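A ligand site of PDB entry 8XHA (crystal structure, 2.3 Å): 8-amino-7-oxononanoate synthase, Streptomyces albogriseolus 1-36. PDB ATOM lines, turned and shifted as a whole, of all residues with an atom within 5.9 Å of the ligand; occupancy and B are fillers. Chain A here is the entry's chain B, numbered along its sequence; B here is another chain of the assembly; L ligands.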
ATOM      1  N   TYR A  53      24.430 -35.386   8.400  1.00  0.00           N
ATOM      2  CA  TYR A  53      24.259 -34.913   7.002  1.00  0.00           C
ATOM      3  C   TYR A  53      25.394 -33.987   6.562  1.00  0.00           C
ATOM      4  O   TYR A  53      25.316 -33.462   5.457  1.00  0.00           O
ATOM      5  CB  TYR A  53      22.841 -34.365   6.752  1.00  0.00           C
ATOM      6  CG  TYR A  53      22.260 -33.389   7.733  1.00  0.00           C
ATOM      7  CD1 TYR A  53      22.825 -32.151   7.956  1.00  0.00           C
ATOM      8  CD2 TYR A  53      21.056 -33.676   8.368  1.00  0.00           C
ATOM      9  CE1 TYR A  53      22.261 -31.247   8.837  1.00  0.00           C
ATOM     10  CE2 TYR A  53      20.471 -32.773   9.242  1.00  0.00           C
ATOM     11  CZ  TYR A  53      21.073 -31.559   9.476  1.00  0.00           C
ATOM     12  OH  TYR A  53      20.506 -30.674  10.346  1.00  0.00           O
ATOM     13  N   ASN A 111      16.778 -18.258   5.144  1.00  0.00           N
ATOM     14  CA  ASN A 111      17.119 -18.909   6.398  1.00  0.00           C
ATOM     15  C   ASN A 111      16.962 -20.429   6.348  1.00  0.00           C
ATOM     16  O   ASN A 111      17.418 -21.112   7.282  1.00  0.00           O
ATOM     17  CB  ASN A 111      16.296 -18.334   7.557  1.00  0.00           C
ATOM     18  CG  ASN A 111      14.813 -18.441   7.320  1.00  0.00           C
ATOM     19  OD1 ASN A 111      14.320 -19.488   6.911  1.00  0.00           O
ATOM     20  ND2 ASN A 111      14.074 -17.349   7.577  1.00  0.00           N
ATOM     21  N   SER A 112      16.350 -20.975   5.303  1.00  0.00           N
ATOM     22  CA  SER A 112      16.274 -22.430   5.188  1.00  0.00           C
ATOM     23  C   SER A 112      15.862 -22.805   3.784  1.00  0.00           C
ATOM     24  O   SER A 112      15.298 -21.999   3.035  1.00  0.00           O
ATOM     25  CB  SER A 112      15.273 -23.028   6.188  1.00  0.00           C
ATOM     26  OG  SER A 112      13.962 -22.671   5.812  1.00  0.00           O
ATOM     27  N   CYS A 113      16.110 -24.086   3.450  1.00  0.00           N
ATOM     28  CA  CYS A 113      15.616 -24.644   2.204  1.00  0.00           C
ATOM     29  C   CYS A 113      14.101 -24.712   2.211  1.00  0.00           C
ATOM     30  O   CYS A 113      13.467 -24.573   1.156  1.00  0.00           O
ATOM     31  CB  CYS A 113      16.200 -26.038   1.951  1.00  0.00           C
ATOM     32  SG  CYS A 113      15.760 -26.788   0.318  1.00  0.00           S
ATOM     33  N   SER A 114      13.498 -24.902   3.384  1.00  0.00           N
ATOM     34  CA  SER A 114      12.043 -24.923   3.473  1.00  0.00           C
ATOM     35  C   SER A 114      11.447 -23.565   3.121  1.00  0.00           C
ATOM     36  O   SER A 114      10.480 -23.488   2.356  1.00  0.00           O
ATOM     37  CB  SER A 114      11.600 -25.366   4.869  1.00  0.00           C
ATOM     38  OG  SER A 114      12.006 -26.697   5.105  1.00  0.00           O
ATOM     39  N   ALA A 115      12.028 -22.487   3.668  1.00  0.00           N
ATOM     40  CA  ALA A 115      11.622 -21.147   3.267  1.00  0.00           C
ATOM     41  C   ALA A 115      11.810 -20.930   1.766  1.00  0.00           C
ATOM     42  O   ALA A 115      11.014 -20.236   1.134  1.00  0.00           O
ATOM     43  CB  ALA A 115      12.402 -20.095   4.037  1.00  0.00           C
ATOM     44  N   HIS A 144      10.349 -34.182  -1.225  1.00  0.00           N
ATOM     45  CA  HIS A 144      10.429 -33.852   0.227  1.00  0.00           C
ATOM     46  C   HIS A 144       9.202 -33.059   0.661  1.00  0.00           C
ATOM     47  O   HIS A 144       8.591 -32.395  -0.180  1.00  0.00           O
ATOM     48  CB  HIS A 144      11.763 -33.160   0.563  1.00  0.00           C
ATOM     49  CG  HIS A 144      12.000 -32.976   2.020  1.00  0.00           C
ATOM     50  ND1 HIS A 144      11.538 -31.887   2.715  1.00  0.00           N
ATOM     51  CD2 HIS A 144      12.654 -33.738   2.909  1.00  0.00           C
ATOM     52  CE1 HIS A 144      11.896 -31.986   3.972  1.00  0.00           C
ATOM     53  NE2 HIS A 144      12.582 -33.108   4.118  1.00  0.00           N
ATOM     54  N   CYS A 146       8.953 -30.410   2.487  1.00  0.00           N
ATOM     55  CA  CYS A 146       9.102 -28.931   2.407  1.00  0.00           C
ATOM     56  C   CYS A 146       8.363 -28.457   1.153  1.00  0.00           C
ATOM     57  O   CYS A 146       7.773 -27.375   1.204  1.00  0.00           O
ATOM     58  CB  CYS A 146      10.571 -28.492   2.411  1.00  0.00           C
ATOM     59  SG  CYS A 146      11.513 -28.839   0.902  1.00  0.00           S
ATOM     60  N   MET A 147       8.353 -29.271   0.102  1.00  0.00           N
ATOM     61  CA  MET A 147       7.664 -28.921  -1.160  1.00  0.00           C
ATOM     62  C   MET A 147       6.256 -29.529  -1.179  1.00  0.00           C
ATOM     63  O   MET A 147       5.316 -28.804  -1.499  1.00  0.00           O
ATOM     64  CB  MET A 147       8.463 -29.459  -2.341  1.00  0.00           C
ATOM     65  CG  MET A 147       9.824 -28.817  -2.497  1.00  0.00           C
ATOM     66  SD  MET A 147      10.854 -29.717  -3.682  1.00  0.00           S
ATOM     67  CE  MET A 147      11.153 -31.230  -2.777  1.00  0.00           C
ATOM     68  N   ASP A 186      13.141 -34.364  -6.168  1.00  0.00           N
ATOM     69  CA  ASP A 186      14.432 -34.279  -5.444  1.00  0.00           C
ATOM     70  C   ASP A 186      15.499 -34.864  -6.361  1.00  0.00           C
ATOM     71  O   ASP A 186      15.230 -35.897  -6.977  1.00  0.00           O
ATOM     72  CB  ASP A 186      14.383 -35.015  -4.107  1.00  0.00           C
ATOM     73  CG  ASP A 186      13.319 -34.529  -3.136  1.00  0.00           C
ATOM     74  OD1 ASP A 186      12.403 -33.834  -3.584  1.00  0.00           O
ATOM     75  OD2 ASP A 186      13.433 -34.856  -1.950  1.00  0.00           O
ATOM     76  N   VAL A 188      18.423 -36.055  -5.495  1.00  0.00           N
ATOM     77  CA  VAL A 188      18.859 -37.298  -4.824  1.00  0.00           C
ATOM     78  C   VAL A 188      17.817 -37.609  -3.757  1.00  0.00           C
ATOM     79  O   VAL A 188      17.494 -36.714  -2.972  1.00  0.00           O
ATOM     80  CB  VAL A 188      20.264 -37.133  -4.204  1.00  0.00           C
ATOM     81  CG1 VAL A 188      20.648 -38.329  -3.353  1.00  0.00           C
ATOM     82  CG2 VAL A 188      21.319 -36.862  -5.271  1.00  0.00           C
ATOM     83  N   SER A 190      16.456 -39.486  -0.385  1.00  0.00           N
ATOM     84  CA  SER A 190      17.028 -39.987   0.860  1.00  0.00           C
ATOM     85  C   SER A 190      16.532 -41.371   1.222  1.00  0.00           C
ATOM     86  O   SER A 190      16.878 -41.878   2.295  1.00  0.00           O
ATOM     87  CB  SER A 190      16.725 -38.993   1.987  1.00  0.00           C
ATOM     88  OG  SER A 190      17.595 -39.174   3.076  1.00  0.00           O
ATOM     89  N   ASP A 215      15.042 -30.292  -5.728  1.00  0.00           N
ATOM     90  CA  ASP A 215      15.537 -30.081  -4.345  1.00  0.00           C
ATOM     91  C   ASP A 215      16.901 -30.758  -4.294  1.00  0.00           C
ATOM     92  O   ASP A 215      16.936 -31.988  -4.429  1.00  0.00           O
ATOM     93  CB  ASP A 215      14.549 -30.607  -3.310  1.00  0.00           C
ATOM     94  CG  ASP A 215      14.968 -30.372  -1.874  1.00  0.00           C
ATOM     95  OD1 ASP A 215      16.166 -30.209  -1.626  1.00  0.00           O
ATOM     96  OD2 ASP A 215      14.073 -30.356  -1.008  1.00  0.00           O
ATOM     97  N   ALA A 217      19.132 -30.714  -1.783  1.00  0.00           N
ATOM     98  CA  ALA A 217      19.700 -30.664  -0.436  1.00  0.00           C
ATOM     99  C   ALA A 217      20.679 -31.805  -0.156  1.00  0.00           C
ATOM    100  O   ALA A 217      21.585 -31.657   0.671  1.00  0.00           O
ATOM    101  CB  ALA A 217      18.569 -30.674   0.599  1.00  0.00           C
ATOM    102  N   HIS A 218      20.502 -32.953  -0.792  1.00  0.00           N
ATOM    103  CA  HIS A 218      21.411 -34.077  -0.612  1.00  0.00           C
ATOM    104  C   HIS A 218      22.314 -34.257  -1.818  1.00  0.00           C
ATOM    105  O   HIS A 218      23.020 -35.259  -1.937  1.00  0.00           O
ATOM    106  CB  HIS A 218      20.630 -35.352  -0.287  1.00  0.00           C
ATOM    107  CG  HIS A 218      19.850 -35.228   0.976  1.00  0.00           C
ATOM    108  ND1 HIS A 218      20.441 -35.329   2.217  1.00  0.00           N
ATOM    109  CD2 HIS A 218      18.542 -34.935   1.199  1.00  0.00           C
ATOM    110  CE1 HIS A 218      19.527 -35.140   3.150  1.00  0.00           C
ATOM    111  NE2 HIS A 218      18.376 -34.904   2.568  1.00  0.00           N
ATOM    112  N   THR A 246      17.966 -25.676  -2.355  1.00  0.00           N
ATOM    113  CA  THR A 246      18.905 -26.546  -1.623  1.00  0.00           C
ATOM    114  C   THR A 246      19.124 -26.061  -0.196  1.00  0.00           C
ATOM    115  O   THR A 246      18.727 -24.931   0.113  1.00  0.00           O
ATOM    116  CB  THR A 246      20.259 -26.667  -2.331  1.00  0.00           C
ATOM    117  OG1 THR A 246      20.968 -27.742  -1.723  1.00  0.00           O
ATOM    118  CG2 THR A 246      21.083 -25.397  -2.247  1.00  0.00           C
ATOM    119  N   SER A 247      19.690 -26.920   0.636  1.00  0.00           N
ATOM    120  CA  SER A 247      20.054 -26.532   2.013  1.00  0.00           C
ATOM    121  C   SER A 247      21.569 -26.346   2.035  1.00  0.00           C
ATOM    122  O   SER A 247      22.249 -27.004   1.253  1.00  0.00           O
ATOM    123  CB  SER A 247      19.596 -27.558   2.990  1.00  0.00           C
ATOM    124  OG  SER A 247      20.093 -27.272   4.286  1.00  0.00           O
ATOM    125  N   LEU A 248      22.060 -25.448   2.884  1.00  0.00           N
ATOM    126  CA  LEU A 248      23.510 -25.176   2.978  1.00  0.00           C
ATOM    127  C   LEU A 248      24.029 -25.632   4.345  1.00  0.00           C
ATOM    128  O   LEU A 248      25.180 -25.339   4.645  1.00  0.00           O
ATOM    129  CB  LEU A 248      23.733 -23.674   2.789  1.00  0.00           C
ATOM    130  CG  LEU A 248      23.255 -23.101   1.459  1.00  0.00           C
ATOM    131  CD1 LEU A 248      23.362 -21.579   1.465  1.00  0.00           C
ATOM    132  CD2 LEU A 248      24.048 -23.680   0.306  1.00  0.00           C
ATOM    133  N   ASN A 249      23.200 -26.338   5.107  1.00  0.00           N
ATOM    134  CA  ASN A 249      23.577 -26.792   6.478  1.00  0.00           C
ATOM    135  C   ASN A 249      24.020 -28.253   6.446  1.00  0.00           C
ATOM    136  O   ASN A 249      24.276 -28.804   7.523  1.00  0.00           O
ATOM    137  CB  ASN A 249      22.454 -26.587   7.488  1.00  0.00           C
ATOM    138  CG  ASN A 249      21.408 -27.678   7.481  1.00  0.00           C
ATOM    139  OD1 ASN A 249      20.871 -28.027   6.439  1.00  0.00           O
ATOM    140  ND2 ASN A 249      21.109 -28.215   8.655  1.00  0.00           N
ATOM    141  N   LYS A 250      24.097 -28.852   5.264  1.00  0.00           N
ATOM    142  CA  LYS A 250      24.454 -30.277   5.159  1.00  0.00           C
ATOM    143  C   LYS A 250      25.891 -30.399   4.647  1.00  0.00           C
ATOM    144  O   LYS A 250      26.808 -30.185   5.429  1.00  0.00           O
ATOM    145  CB  LYS A 250      23.428 -30.985   4.274  1.00  0.00           C
ATOM    146  CG  LYS A 250      21.976 -30.831   4.706  1.00  0.00           C
ATOM    147  CD  LYS A 250      21.009 -31.611   3.838  1.00  0.00           C
ATOM    148  CE  LYS A 250      19.554 -31.294   4.113  1.00  0.00           C
ATOM    149  NZ  LYS A 250      19.196 -31.544   5.525  1.00  0.00           N
ATOM    150  N   GLY A 256      21.313 -22.371   6.641  1.00  0.00           N
ATOM    151  CA  GLY A 256      20.320 -21.747   5.754  1.00  0.00           C
ATOM    152  C   GLY A 256      20.081 -22.522   4.489  1.00  0.00           C
ATOM    153  O   GLY A 256      20.461 -23.702   4.422  1.00  0.00           O
ATOM    154  N   GLY A 257      19.447 -21.872   3.515  1.00  0.00           N
ATOM    155  CA  GLY A 257      19.161 -22.513   2.237  1.00  0.00           C
ATOM    156  C   GLY A 257      19.337 -21.523   1.102  1.00  0.00           C
ATOM    157  O   GLY A 257      19.846 -20.433   1.347  1.00  0.00           O
ATOM    158  N   ASN B 111      13.940 -21.628  13.035  1.00  0.00           N
ATOM    159  CA  ASN B 111      14.810 -20.694  12.346  1.00  0.00           C
ATOM    160  C   ASN B 111      14.104 -19.385  11.968  1.00  0.00           C
ATOM    161  O   ASN B 111      14.771 -18.466  11.473  1.00  0.00           O
ATOM    162  CB  ASN B 111      15.414 -21.361  11.107  1.00  0.00           C
ATOM    163  CG  ASN B 111      14.374 -22.033  10.237  1.00  0.00           C
ATOM    164  OD1 ASN B 111      13.362 -21.422   9.894  1.00  0.00           O
ATOM    165  ND2 ASN B 111      14.615 -23.299   9.870  1.00  0.00           N
ATOM    166  N   TRP B 282      11.341 -31.271  10.236  1.00  0.00           N
ATOM    167  CA  TRP B 282      12.333 -31.472   9.180  1.00  0.00           C
ATOM    168  C   TRP B 282      12.973 -30.178   8.654  1.00  0.00           C
ATOM    169  O   TRP B 282      13.542 -30.187   7.558  1.00  0.00           O
ATOM    170  CB  TRP B 282      11.726 -32.269   8.024  1.00  0.00           C
ATOM    171  CG  TRP B 282      10.303 -31.971   7.641  1.00  0.00           C
ATOM    172  CD1 TRP B 282       9.237 -32.832   7.748  1.00  0.00           C
ATOM    173  CD2 TRP B 282       9.790 -30.764   7.040  1.00  0.00           C
ATOM    174  NE1 TRP B 282       8.091 -32.230   7.271  1.00  0.00           N
ATOM    175  CE2 TRP B 282       8.402 -30.966   6.831  1.00  0.00           C
ATOM    176  CE3 TRP B 282      10.358 -29.542   6.656  1.00  0.00           C
ATOM    177  CZ2 TRP B 282       7.577 -29.979   6.260  1.00  0.00           C
ATOM    178  CZ3 TRP B 282       9.531 -28.566   6.105  1.00  0.00           C
ATOM    179  CH2 TRP B 282       8.159 -28.794   5.899  1.00  0.00           C
ATOM    180  N   SER B 283      12.920 -29.075   9.398  1.00  0.00           N
ATOM    181  CA  SER B 283      13.675 -27.889   9.026  1.00  0.00           C
ATOM    182  C   SER B 283      14.750 -27.602  10.078  1.00  0.00           C
ATOM    183  O   SER B 283      14.539 -27.815  11.277  1.00  0.00           O
ATOM    184  CB  SER B 283      12.784 -26.658   8.845  1.00  0.00           C
ATOM    185  OG  SER B 283      13.466 -25.698   8.041  1.00  0.00           O
ATOM    186  N   GLN B 284      15.889 -27.110   9.579  1.00  0.00           N
ATOM    187  CA  GLN B 284      17.086 -26.923  10.428  1.00  0.00           C
ATOM    188  C   GLN B 284      16.866 -26.103  11.698  1.00  0.00           C
ATOM    189  O   GLN B 284      16.137 -25.110  11.656  1.00  0.00           O
ATOM    190  CB  GLN B 284      18.216 -26.296   9.609  1.00  0.00           C
ATOM    191  CG  GLN B 284      17.813 -25.091   8.766  1.00  0.00           C
ATOM    192  CD  GLN B 284      18.978 -24.613   7.935  1.00  0.00           C
ATOM    193  OE1 GLN B 284      19.993 -24.178   8.459  1.00  0.00           O
ATOM    194  NE2 GLN B 284      18.838 -24.711   6.625  1.00  0.00           N
HETATM  195  N1  LIG L   1      14.944 -30.940   1.394  1.00  0.00           N
HETATM  196  C1  LIG L   1      15.435 -32.195   1.690  1.00  0.00           C
HETATM  197  C2  LIG L   1      15.585 -33.193   0.573  1.00  0.00           C
HETATM  198  C3  LIG L   1      15.765 -32.514   3.013  1.00  0.00           C
HETATM  199  O1  LIG L   1      16.252 -33.740   3.351  1.00  0.00           O
HETATM  200  C4  LIG L   1      15.614 -31.574   4.012  1.00  0.00           C
HETATM  201  C5  LIG L   1      16.068 -31.886   5.412  1.00  0.00           C
HETATM  202  O2  LIG L   1      15.500 -32.718   6.127  1.00  0.00           O
HETATM  203  C6  LIG L   1      15.113 -30.315   3.702  1.00  0.00           C
HETATM  204  C7  LIG L   1      14.782 -30.004   2.385  1.00  0.00           C
HETATM  205  C8  LIG L   1      14.951 -29.274   4.792  1.00  0.00           C
HETATM  206  O3  LIG L   1      15.886 -28.224   4.586  1.00  0.00           O
HETATM  207  P1  LIG L   1      16.012 -27.043   5.666  1.00  0.00           P
HETATM  208  O4  LIG L   1      17.111 -26.141   5.164  1.00  0.00           O
HETATM  209  O5  LIG L   1      14.703 -26.292   5.788  1.00  0.00           O
HETATM  210  O6  LIG L   1      16.358 -27.558   7.047  1.00  0.00           O
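An oxygen (O4) of the ligand sits at hydrogen-bond distance from the side-chain amide nitrogen of Gln 284 of chain B, at 2.7 Å. N1 of the ligand sits at hydrogen-bond distance from OD2 of Asp 215 (2.6 Å). O1 of the ligand lies within hydrogen-bond range of NE2 of His 218, 2.5 Å away. An oxygen (O5) of the ligand sits at hydrogen-bond distance from the backbone NH of Ser 114, 3.0 Å away. The backbone NH (N) of Cys 113 sits at hydrogen-bond distance from an oxygen (O4) of the ligand, at 2.9 Å. The side-chain hydroxyl (OG) of Ser 114 lies within hydrogen-bond range of an oxygen (O5) of the ligand (2.8 Å). An oxygen (O5) of the ligand lies within hydrogen-bond range of the side-chain hydroxyl (OG) of Ser 283 of chain B (2.6 Å). O4 of the ligand lies within hydrogen-bond range of OG of Ser 247, 3.3 Å away. An oxygen (O6) of the ligand is in hydrogen-bond range of the backbone NH (N) of Gln 284 of chain B (2.6 Å).
Ser 112 touches the ligand. CD2 of His 144 touches C3 of the ligand (3.3 Å). Cys 146 touches the ligand. Asp 186 touches the ligand. Ala 217 touches the ligand (CB to C1, 3.7 Å). Lys 250 touches the ligand. Trp 282 of chain B touches the ligand (O to C8, 3.2 Å). The nearest printed residue that does not touch the ligand is Gly 256 (4.2 Å).
The side-chain carboxylate of Asp 186 lies within hydrogen-bond range of the backbone NH of His 144 (3.1 Å). The side-chain sulfur (SG) of Cys 113 lies close to the backbone carbonyl oxygen (O) of Thr 246 (3.5 Å). The side-chain hydroxyl (OG) of Ser 247 lies within hydrogen-bond range of the side-chain amide oxygen (OD1) of Asn 249 (2.4 Å). The side-chain hydroxyl (OG) of Ser 114 is in hydrogen-bond range of the side-chain hydroxyl (OG) of Ser 283 of chain B. OG of Ser 112 lies within hydrogen-bond range of N of Ala 115 (2.9 Å). The backbone NH of Ala 217 lies close to the side-chain hydroxyl of Thr 246, 3.5 Å away. A ring nitrogen (ND1) of His 144 is in hydrogen-bond range of the backbone NH of Cys 146 (3.0 Å). N of Ala 217 lies within hydrogen-bond range of OD1 of Asp 215 (3.0 Å).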
